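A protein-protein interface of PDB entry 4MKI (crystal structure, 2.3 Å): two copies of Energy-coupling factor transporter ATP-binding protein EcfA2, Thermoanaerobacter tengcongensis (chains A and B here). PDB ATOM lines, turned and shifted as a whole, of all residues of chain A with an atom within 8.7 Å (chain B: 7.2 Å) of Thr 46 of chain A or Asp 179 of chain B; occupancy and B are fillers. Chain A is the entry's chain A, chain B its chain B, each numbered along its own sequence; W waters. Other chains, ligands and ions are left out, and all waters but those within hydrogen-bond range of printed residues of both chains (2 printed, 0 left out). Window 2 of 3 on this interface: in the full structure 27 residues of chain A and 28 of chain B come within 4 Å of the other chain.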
ATOM      1  N   ILE A  43      -5.838 -24.242  14.884  1.00  0.00           N
ATOM      2  CA  ILE A  43      -6.422 -23.319  15.799  1.00  0.00           C
ATOM      3  C   ILE A  43      -7.279 -24.067  16.785  1.00  0.00           C
ATOM      4  O   ILE A  43      -7.636 -25.244  16.604  1.00  0.00           O
ATOM      5  CB  ILE A  43      -7.255 -22.291  15.062  1.00  0.00           C
ATOM      6  CG1 ILE A  43      -8.402 -22.964  14.310  1.00  0.00           C
ATOM      7  CG2 ILE A  43      -6.384 -21.509  14.081  1.00  0.00           C
ATOM      8  CD1 ILE A  43      -9.275 -21.960  13.662  1.00  0.00           C
ATOM      9  N   GLY A  44      -7.581 -23.421  17.886  1.00  0.00           N
ATOM     10  CA  GLY A  44      -8.479 -23.993  18.881  1.00  0.00           C
ATOM     11  C   GLY A  44      -8.321 -23.296  20.212  1.00  0.00           C
ATOM     12  O   GLY A  44      -7.281 -22.692  20.486  1.00  0.00           O
ATOM     13  N   HIS A  45      -9.304 -23.458  21.080  1.00  0.00           N
ATOM     14  CA  HIS A  45      -9.263 -22.799  22.373  1.00  0.00           C
ATOM     15  C   HIS A  45      -8.098 -23.271  23.228  1.00  0.00           C
ATOM     16  O   HIS A  45      -7.568 -24.341  23.047  1.00  0.00           O
ATOM     17  CB  HIS A  45     -10.626 -22.952  23.117  1.00  0.00           C
ATOM     18  CG  HIS A  45     -10.953 -24.345  23.523  1.00  0.00           C
ATOM     19  ND1 HIS A  45     -10.443 -24.928  24.648  1.00  0.00           N
ATOM     20  CD2 HIS A  45     -11.748 -25.283  22.945  1.00  0.00           C
ATOM     21  CE1 HIS A  45     -10.864 -26.179  24.732  1.00  0.00           C
ATOM     22  NE2 HIS A  45     -11.646 -26.416  23.703  1.00  0.00           N
ATOM     23  N   THR A  46      -7.738 -22.467  24.205  1.00  0.00           N
ATOM     24  CA  THR A  46      -6.787 -22.858  25.206  1.00  0.00           C
ATOM     25  C   THR A  46      -7.235 -24.141  25.892  1.00  0.00           C
ATOM     26  O   THR A  46      -8.377 -24.244  26.331  1.00  0.00           O
ATOM     27  CB  THR A  46      -6.665 -21.777  26.304  1.00  0.00           C
ATOM     28  OG1 THR A  46      -6.524 -20.506  25.685  1.00  0.00           O
ATOM     29  CG2 THR A  46      -5.428 -22.034  27.205  1.00  0.00           C
ATOM     30  N   GLY A  47      -6.345 -25.121  25.973  1.00  0.00           N
ATOM     31  CA  GLY A  47      -6.706 -26.449  26.486  1.00  0.00           C
ATOM     32  C   GLY A  47      -7.542 -27.316  25.545  1.00  0.00           C
ATOM     33  O   GLY A  47      -8.167 -28.224  25.997  1.00  0.00           O
ATOM     34  N   SER A  48      -7.472 -27.095  24.222  1.00  0.00           N
ATOM     35  CA  SER A  48      -8.091 -27.952  23.205  1.00  0.00           C
ATOM     36  C   SER A  48      -7.204 -29.077  22.707  1.00  0.00           C
ATOM     37  O   SER A  48      -7.638 -29.897  21.886  1.00  0.00           O
ATOM     38  CB  SER A  48      -8.567 -27.080  21.987  1.00  0.00           C
ATOM     39  OG  SER A  48      -7.503 -26.394  21.342  1.00  0.00           O
ATOM     40  N   GLY A  49      -5.932 -29.067  23.087  1.00  0.00           N
ATOM     41  CA  GLY A  49      -5.037 -30.117  22.691  1.00  0.00           C
ATOM     42  C   GLY A  49      -4.011 -29.851  21.629  1.00  0.00           C
ATOM     43  O   GLY A  49      -3.327 -30.793  21.192  1.00  0.00           O
ATOM     44  N   LYS A  50      -3.843 -28.591  21.237  1.00  0.00           N
ATOM     45  CA  LYS A  50      -2.961 -28.229  20.129  1.00  0.00           C
ATOM     46  C   LYS A  50      -1.516 -28.565  20.410  1.00  0.00           C
ATOM     47  O   LYS A  50      -0.863 -29.229  19.631  1.00  0.00           O
ATOM     48  CB  LYS A  50      -3.095 -26.756  19.863  1.00  0.00           C
ATOM     49  CG  LYS A  50      -4.446 -26.341  19.368  1.00  0.00           C
ATOM     50  CD  LYS A  50      -4.512 -24.842  19.202  1.00  0.00           C
ATOM     51  CE  LYS A  50      -4.928 -24.268  20.560  1.00  0.00           C
ATOM     52  NZ  LYS A  50      -3.955 -23.334  21.029  1.00  0.00           N
ATOM     53  N   SER A  51      -1.042 -28.179  21.585  1.00  0.00           N
ATOM     54  CA  SER A  51       0.271 -28.496  22.019  1.00  0.00           C
ATOM     55  C   SER A  51       0.487 -30.014  22.185  1.00  0.00           C
ATOM     56  O   SER A  51       1.489 -30.587  21.754  1.00  0.00           O
ATOM     57  CB  SER A  51       0.546 -27.757  23.325  1.00  0.00           C
ATOM     58  OG  SER A  51       1.829 -28.148  23.748  1.00  0.00           O
ATOM     59  N   GLU A 173       2.879 -20.321  17.489  1.00  0.00           N
ATOM     60  CA  GLU A 173       2.759 -18.833  17.599  1.00  0.00           C
ATOM     61  C   GLU A 173       4.061 -18.041  17.368  1.00  0.00           C
ATOM     62  O   GLU A 173       4.559 -17.352  18.271  1.00  0.00           O
ATOM     63  CB  GLU A 173       2.151 -18.430  18.938  1.00  0.00           C
ATOM     64  CG  GLU A 173       1.485 -17.073  18.902  1.00  0.00           C
ATOM     65  CD  GLU A 173       0.167 -17.127  18.157  1.00  0.00           C
ATOM     66  OE1 GLU A 173      -0.844 -17.504  18.793  1.00  0.00           O
ATOM     67  OE2 GLU A 173       0.166 -16.831  16.951  1.00  0.00           O
ATOM     68  N   SER A 205      -1.699 -21.125  16.154  1.00  0.00           N
ATOM     69  CA  SER A 205      -1.910 -19.719  16.399  1.00  0.00           C
ATOM     70  C   SER A 205      -3.322 -19.347  16.818  1.00  0.00           C
ATOM     71  O   SER A 205      -4.309 -19.880  16.318  1.00  0.00           O
ATOM     72  CB  SER A 205      -1.530 -18.921  15.129  1.00  0.00           C
ATOM     73  OG  SER A 205      -1.746 -17.505  15.312  1.00  0.00           O
ATOM     74  N   HIS A 206      -3.395 -18.363  17.686  1.00  0.00           N
ATOM     75  CA  HIS A 206      -4.622 -17.742  18.046  1.00  0.00           C
ATOM     76  C   HIS A 206      -4.976 -16.545  17.156  1.00  0.00           C
ATOM     77  O   HIS A 206      -5.974 -15.885  17.374  1.00  0.00           O
ATOM     78  CB  HIS A 206      -4.530 -17.271  19.485  1.00  0.00           C
ATOM     79  CG  HIS A 206      -4.534 -18.380  20.487  1.00  0.00           C
ATOM     80  ND1 HIS A 206      -5.369 -19.463  20.372  1.00  0.00           N
ATOM     81  CD2 HIS A 206      -3.806 -18.579  21.611  1.00  0.00           C
ATOM     82  CE1 HIS A 206      -5.163 -20.281  21.387  1.00  0.00           C
ATOM     83  NE2 HIS A 206      -4.214 -19.773  22.148  1.00  0.00           N
ATOM     84  N   ASN A 207      -4.180 -16.230  16.157  1.00  0.00           N
ATOM     85  CA  ASN A 207      -4.485 -15.057  15.347  1.00  0.00           C
ATOM     86  C   ASN A 207      -5.189 -15.517  14.084  1.00  0.00           C
ATOM     87  O   ASN A 207      -4.544 -16.059  13.183  1.00  0.00           O
ATOM     88  CB  ASN A 207      -3.197 -14.301  14.988  1.00  0.00           C
ATOM     89  CG  ASN A 207      -3.446 -13.004  14.237  1.00  0.00           C
ATOM     90  OD1 ASN A 207      -4.058 -12.982  13.195  1.00  0.00           O
ATOM     91  ND2 ASN A 207      -2.965 -11.926  14.778  1.00  0.00           N
ATOM     92  N   MET A 208      -6.491 -15.248  14.016  1.00  0.00           N
ATOM     93  CA  MET A 208      -7.353 -15.773  13.006  1.00  0.00           C
ATOM     94  C   MET A 208      -7.038 -15.141  11.650  1.00  0.00           C
ATOM     95  O   MET A 208      -7.042 -15.819  10.653  1.00  0.00           O
ATOM     96  CB  MET A 208      -8.815 -15.539  13.417  1.00  0.00           C
ATOM     97  CG  MET A 208      -9.254 -16.219  14.704  1.00  0.00           C
ATOM     98  SD  MET A 208      -9.124 -18.007  14.746  1.00  0.00           S
ATOM     99  CE  MET A 208      -7.512 -18.287  15.474  1.00  0.00           C
ATOM    100  N   MET A 221      -9.383 -27.570  16.562  1.00  0.00           N
ATOM    101  CA  MET A 221      -9.450 -28.484  17.725  1.00  0.00           C
ATOM    102  C   MET A 221     -10.566 -28.001  18.630  1.00  0.00           C
ATOM    103  O   MET A 221     -10.877 -26.802  18.691  1.00  0.00           O
ATOM    104  CB  MET A 221      -8.163 -28.450  18.521  1.00  0.00           C
ATOM    105  CG  MET A 221      -6.888 -28.794  17.766  1.00  0.00           C
ATOM    106  SD  MET A 221      -6.893 -30.506  17.359  1.00  0.00           S
ATOM    107  CE  MET A 221      -6.441 -31.256  18.932  1.00  0.00           C
ATOM    108  N   ASN A 222     -11.140 -28.918  19.389  1.00  0.00           N
ATOM    109  CA  ASN A 222     -12.170 -28.556  20.373  1.00  0.00           C
ATOM    110  C   ASN A 222     -12.205 -29.663  21.395  1.00  0.00           C
ATOM    111  O   ASN A 222     -12.438 -30.820  21.081  1.00  0.00           O
ATOM    112  CB  ASN A 222     -13.505 -28.335  19.699  1.00  0.00           C
ATOM    113  CG  ASN A 222     -14.626 -28.045  20.682  1.00  0.00           C
ATOM    114  OD1 ASN A 222     -14.461 -27.310  21.667  1.00  0.00           O
ATOM    115  ND2 ASN A 222     -15.773 -28.616  20.421  1.00  0.00           N
ATOM    116  N   ARG A 223     -11.805 -29.312  22.607  1.00  0.00           N
ATOM    117  CA  ARG A 223     -11.757 -30.234  23.730  1.00  0.00           C
ATOM    118  C   ARG A 223     -11.094 -31.552  23.437  1.00  0.00           C
ATOM    119  O   ARG A 223     -11.616 -32.592  23.796  1.00  0.00           O
ATOM    120  CB  ARG A 223     -13.136 -30.438  24.309  1.00  0.00           C
ATOM    121  CG  ARG A 223     -13.531 -29.144  24.946  1.00  0.00           C
ATOM    122  CD  ARG A 223     -14.970 -29.144  25.219  1.00  0.00           C
ATOM    123  NE  ARG A 223     -15.377 -27.867  25.780  1.00  0.00           N
ATOM    124  CZ  ARG A 223     -15.348 -27.580  27.085  1.00  0.00           C
ATOM    125  NH1 ARG A 223     -14.874 -28.456  27.972  1.00  0.00           N
ATOM    126  NH2 ARG A 223     -15.825 -26.417  27.514  1.00  0.00           N
ATOM    127  N   GLY A 224      -9.931 -31.492  22.803  1.00  0.00           N
ATOM    128  CA  GLY A 224      -9.199 -32.704  22.525  1.00  0.00           C
ATOM    129  C   GLY A 224      -9.621 -33.415  21.247  1.00  0.00           C
ATOM    130  O   GLY A 224      -9.075 -34.469  20.923  1.00  0.00           O
ATOM    131  N   ILE A 245     -16.920 -22.240  20.232  1.00  0.00           N
ATOM    132  CA  ILE A 245     -15.838 -23.071  20.765  1.00  0.00           C
ATOM    133  C   ILE A 245     -14.561 -22.284  21.093  1.00  0.00           C
ATOM    134  O   ILE A 245     -13.476 -22.840  21.161  1.00  0.00           O
ATOM    135  CB  ILE A 245     -15.536 -24.243  19.840  1.00  0.00           C
ATOM    136  CG1 ILE A 245     -15.093 -23.765  18.437  1.00  0.00           C
ATOM    137  CG2 ILE A 245     -16.765 -25.137  19.740  1.00  0.00           C
ATOM    138  CD1 ILE A 245     -14.705 -24.897  17.529  1.00  0.00           C
ATOM    139  N   GLY A 246     -14.699 -20.991  21.337  1.00  0.00           N
ATOM    140  CA  GLY A 246     -13.592 -20.190  21.874  1.00  0.00           C
ATOM    141  C   GLY A 246     -12.810 -19.428  20.835  1.00  0.00           C
ATOM    142  O   GLY A 246     -11.913 -18.712  21.174  1.00  0.00           O
ATOM    143  N   LEU A 247     -13.203 -19.533  19.572  1.00  0.00           N
ATOM    144  CA  LEU A 247     -12.498 -18.904  18.469  1.00  0.00           C
ATOM    145  C   LEU A 247     -13.249 -17.691  17.871  1.00  0.00           C
ATOM    146  O   LEU A 247     -14.127 -17.129  18.472  1.00  0.00           O
ATOM    147  CB  LEU A 247     -12.261 -19.967  17.416  1.00  0.00           C
ATOM    148  CG  LEU A 247     -11.505 -21.205  17.907  1.00  0.00           C
ATOM    149  CD1 LEU A 247     -11.393 -22.229  16.804  1.00  0.00           C
ATOM    150  CD2 LEU A 247     -10.129 -20.760  18.384  1.00  0.00           C
ATOM    151  N   SER A 248     -12.913 -17.340  16.659  1.00  0.00           N
ATOM    152  CA  SER A 248     -13.353 -16.116  16.068  1.00  0.00           C
ATOM    153  C   SER A 248     -13.068 -16.195  14.570  1.00  0.00           C
ATOM    154  O   SER A 248     -12.391 -17.125  14.116  1.00  0.00           O
ATOM    155  CB  SER A 248     -12.539 -14.986  16.654  1.00  0.00           C
ATOM    156  OG  SER A 248     -13.040 -13.786  16.165  1.00  0.00           O
ATOM    157  N   GLY B 150      -3.678 -21.300  33.894  1.00  0.00           N
ATOM    158  CA  GLY B 150      -2.936 -20.085  33.506  1.00  0.00           C
ATOM    159  C   GLY B 150      -3.795 -18.844  33.485  1.00  0.00           C
ATOM    160  O   GLY B 150      -3.415 -17.813  34.011  1.00  0.00           O
ATOM    161  N   GLY B 151      -5.006 -18.970  32.942  1.00  0.00           N
ATOM    162  CA  GLY B 151      -5.956 -17.876  32.919  1.00  0.00           C
ATOM    163  C   GLY B 151      -6.465 -17.445  34.297  1.00  0.00           C
ATOM    164  O   GLY B 151      -6.623 -16.237  34.607  1.00  0.00           O
ATOM    165  N   THR B 175      -3.696  -9.149  26.741  1.00  0.00           N
ATOM    166  CA  THR B 175      -4.292 -10.249  26.007  1.00  0.00           C
ATOM    167  C   THR B 175      -3.269 -11.286  25.583  1.00  0.00           C
ATOM    168  O   THR B 175      -3.643 -12.293  24.972  1.00  0.00           O
ATOM    169  CB  THR B 175      -5.005  -9.792  24.732  1.00  0.00           C
ATOM    170  OG1 THR B 175      -4.047  -9.204  23.834  1.00  0.00           O
ATOM    171  CG2 THR B 175      -6.117  -8.815  25.076  1.00  0.00           C
ATOM    172  N   ALA B 176      -1.998 -11.060  25.917  1.00  0.00           N
ATOM    173  CA  ALA B 176      -0.921 -11.939  25.454  1.00  0.00           C
ATOM    174  C   ALA B 176      -1.150 -13.424  25.802  1.00  0.00           C
ATOM    175  O   ALA B 176      -1.321 -13.770  26.951  1.00  0.00           O
ATOM    176  CB  ALA B 176       0.388 -11.462  26.060  1.00  0.00           C
ATOM    177  N   GLY B 177      -1.143 -14.290  24.797  1.00  0.00           N
ATOM    178  CA  GLY B 177      -1.146 -15.721  25.016  1.00  0.00           C
ATOM    179  C   GLY B 177      -2.549 -16.277  25.074  1.00  0.00           C
ATOM    180  O   GLY B 177      -2.763 -17.474  25.108  1.00  0.00           O
ATOM    181  N   LEU B 178      -3.535 -15.411  25.051  1.00  0.00           N
ATOM    182  CA  LEU B 178      -4.884 -15.855  25.200  1.00  0.00           C
ATOM    183  C   LEU B 178      -5.550 -16.251  23.905  1.00  0.00           C
ATOM    184  O   LEU B 178      -5.175 -15.800  22.829  1.00  0.00           O
ATOM    185  CB  LEU B 178      -5.714 -14.736  25.850  1.00  0.00           C
ATOM    186  CG  LEU B 178      -5.275 -14.294  27.241  1.00  0.00           C
ATOM    187  CD1 LEU B 178      -6.216 -13.199  27.717  1.00  0.00           C
ATOM    188  CD2 LEU B 178      -5.248 -15.454  28.210  1.00  0.00           C
ATOM    189  N   ASP B 179      -6.542 -17.129  24.004  1.00  0.00           N
ATOM    190  CA  ASP B 179      -7.313 -17.519  22.829  1.00  0.00           C
ATOM    191  C   ASP B 179      -8.245 -16.388  22.446  1.00  0.00           C
ATOM    192  O   ASP B 179      -8.383 -15.433  23.209  1.00  0.00           O
ATOM    193  CB  ASP B 179      -8.008 -18.878  23.017  1.00  0.00           C
ATOM    194  CG  ASP B 179      -9.092 -18.877  24.067  1.00  0.00           C
ATOM    195  OD1 ASP B 179      -9.580 -17.802  24.454  1.00  0.00           O
ATOM    196  OD2 ASP B 179      -9.514 -20.009  24.435  1.00  0.00           O
ATOM    197  N   PRO B 180      -8.833 -16.442  21.255  1.00  0.00           N
ATOM    198  CA  PRO B 180      -9.630 -15.292  20.869  1.00  0.00           C
ATOM    199  C   PRO B 180     -10.773 -14.915  21.761  1.00  0.00           C
ATOM    200  O   PRO B 180     -11.068 -13.728  21.932  1.00  0.00           O
ATOM    201  CB  PRO B 180     -10.141 -15.669  19.506  1.00  0.00           C
ATOM    202  CG  PRO B 180      -9.056 -16.602  18.949  1.00  0.00           C
ATOM    203  CD  PRO B 180      -8.737 -17.413  20.167  1.00  0.00           C
ATOM    204  N   LYS B 181     -11.420 -15.874  22.380  1.00  0.00           N
ATOM    205  CA  LYS B 181     -12.463 -15.526  23.345  1.00  0.00           C
ATOM    206  C   LYS B 181     -11.819 -14.898  24.587  1.00  0.00           C
ATOM    207  O   LYS B 181     -12.367 -13.980  25.159  1.00  0.00           O
ATOM    208  CB  LYS B 181     -13.299 -16.752  23.682  1.00  0.00           C
ATOM    209  CG  LYS B 181     -13.991 -16.758  25.053  1.00  0.00           C
ATOM    210  CD  LYS B 181     -14.604 -18.166  25.304  1.00  0.00           C
ATOM    211  CE  LYS B 181     -14.697 -18.615  26.755  1.00  0.00           C
ATOM    212  NZ  LYS B 181     -16.028 -18.358  27.365  1.00  0.00           N
ATOM    213  N   GLY B 182     -10.670 -15.421  25.013  1.00  0.00           N
ATOM    214  CA  GLY B 182      -9.961 -14.913  26.134  1.00  0.00           C
ATOM    215  C   GLY B 182      -9.625 -13.449  25.930  1.00  0.00           C
ATOM    216  O   GLY B 182      -9.715 -12.632  26.862  1.00  0.00           O
ATOM    217  N   LYS B 183      -9.181 -13.132  24.728  1.00  0.00           N
ATOM    218  CA  LYS B 183      -8.718 -11.803  24.437  1.00  0.00           C
ATOM    219  C   LYS B 183      -9.878 -10.841  24.585  1.00  0.00           C
ATOM    220  O   LYS B 183      -9.734  -9.827  25.283  1.00  0.00           O
ATOM    221  CB  LYS B 183      -8.147 -11.717  23.037  1.00  0.00           C
ATOM    222  CG  LYS B 183      -6.805 -12.415  22.859  1.00  0.00           C
ATOM    223  CD  LYS B 183      -6.573 -12.649  21.376  1.00  0.00           C
ATOM    224  CE  LYS B 183      -5.251 -13.252  21.005  1.00  0.00           C
ATOM    225  NZ  LYS B 183      -4.212 -12.392  21.644  1.00  0.00           N
ATOM    226  N   GLN B 184     -11.022 -11.178  23.980  1.00  0.00           N
ATOM    227  CA  GLN B 184     -12.221 -10.296  24.073  1.00  0.00           C
ATOM    228  C   GLN B 184     -12.682 -10.195  25.532  1.00  0.00           C
ATOM    229  O   GLN B 184     -13.034  -9.142  26.009  1.00  0.00           O
ATOM    230  CB  GLN B 184     -13.388 -10.742  23.157  1.00  0.00           C
ATOM    231  CG  GLN B 184     -13.047 -10.957  21.645  1.00  0.00           C
ATOM    232  CD  GLN B 184     -14.153 -11.660  20.815  1.00  0.00           C
ATOM    233  OE1 GLN B 184     -15.331 -11.265  20.870  1.00  0.00           O
ATOM    234  NE2 GLN B 184     -13.774 -12.681  20.028  1.00  0.00           N
ATOM    235  N   GLU B 185     -12.638 -11.289  26.257  1.00  0.00           N
ATOM    236  CA  GLU B 185     -13.102 -11.227  27.636  1.00  0.00           C
ATOM    237  C   GLU B 185     -12.219 -10.319  28.508  1.00  0.00           C
ATOM    238  O   GLU B 185     -12.740  -9.546  29.301  1.00  0.00           O
ATOM    239  CB  GLU B 185     -13.198 -12.615  28.258  1.00  0.00           C
ATOM    240  CG  GLU B 185     -13.628 -12.572  29.709  1.00  0.00           C
ATOM    241  CD  GLU B 185     -13.667 -13.932  30.378  1.00  0.00           C
ATOM    242  OE1 GLU B 185     -13.396 -14.968  29.704  1.00  0.00           O
ATOM    243  OE2 GLU B 185     -13.971 -13.927  31.596  1.00  0.00           O
HETATM  244  O   HOH W   1      -3.883 -20.015  25.101  1.00  0.00           O
HETATM  245  O   HOH W   2     -15.414 -14.432  19.552  1.00  0.00           O
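CB of His 45 of chain A touches OD2 of Asp 179 of chain B (3.4 Å).
CD2 of His 206 of chain A touches O of Gly 177 of chain B, 3.8 Å away.
His 206 of chain A touches Leu 178 of chain B.
Asp 179 of chain B touches His 206 of chain A.
His 206 of chain A touches Pro 180 of chain B.
Gly 246 of chain A touches Pro 180 of chain B (O to CD, 3.6 Å).
CB of Ser 248 of chain A touches CB of Pro 180 of chain B, at 3.8 Å.
Printed residues of chain A that touch a printed residue of chain B: His 45, Thr 46, His 206, Gly 246 and Ser 248.
Hydrophobic or aromatic side chains of chain A that line the printed part of chain B: His 45 and His 206.
Of the 13 printed residues of chain B, 5 touch a printed residue of chain A.
Hydrophobic or aromatic side chains of chain B within 4 Å of the printed part of chain A: Pro 180.
Among the printed residues, 9 pairs touch across the chains.
Among the printed residues, no Asp or Glu carboxylate lies within 4 Å of a Lys or Arg side-chain nitrogen of the other chain.
No position is printed for both chains.
Water W2 bridges NE2 of Gln 184 of chain B (2.4 Å) and O of Leu 247 of chain A (3.2 Å).
Water W1 lies within hydrogen-bond range of the side-chain hydroxyl of Thr 46 of chain A, the backbone carbonyl oxygen of Gly 177 of chain B and a ring nitrogen (NE2) of His 206 of chain A.
The backbone NH (N) of Thr 46 of chain A lies within hydrogen-bond range of the side-chain carboxylate (OD2) of Asp 179 of chain B (3.0 Å).
The backbone carbonyl oxygen (O) of Gly 246 of chain A is in hydrogen-bond range of the backbone NH (N) of Lys 181 of chain B, at 3.1 Å.
The backbone carbonyl oxygen (O) of His 45 of chain A sits at hydrogen-bond distance from the side-chain hydroxyl (OG) of Ser 48 of chain A (2.7 Å).
The side-chain carboxylate (OD1) of Asp 179 of chain B is in hydrogen-bond range of the backbone NH (N) of Gly 182 of chain B.
The backbone carbonyl oxygen (O) of Pro 180 of chain B sits close to the side-chain amide nitrogen (NE2) of Gln 184 of chain B (3.5 Å).
N of Arg 223 of chain A sits at hydrogen-bond distance from NE2 of His 45 of chain A, 3.1 Å away.
The backbone NH of His 206 of chain A sits at hydrogen-bond distance from the side-chain carboxylate of Glu 173 of chain A (2.9 Å).
OD1 of Asp 179 of chain B sits close to N of Lys 181 of chain B (3.4 Å).
Of the printed residues of chain B, His 45 of chain A touches Asp 179 (3.4 Å).
Thr 46 of chain A touches just one residue of chain B: Asp 179.
Of the printed residues of chain B, His 206 of chain A touches Gly 177, Leu 178, Asp 179 and Pro 180.
Asp 179 of chain B touches just these residues of chain A: His 45 (3.4 Å), Thr 46 (3.0 Å) and His 206 (3.6 Å).
Pro 180 of chain B touches just these residues of chain A: His 206 (3.5 Å), Gly 246 (3.6 Å) and Ser 248 (3.8 Å).
Printed residues of chain A within 4 Å of Lys 181 of chain B: Gly 246.
The nearest printed residue of chain A that does not touch Lys 181 of chain B is Leu 247 of chain A (4.9 Å).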
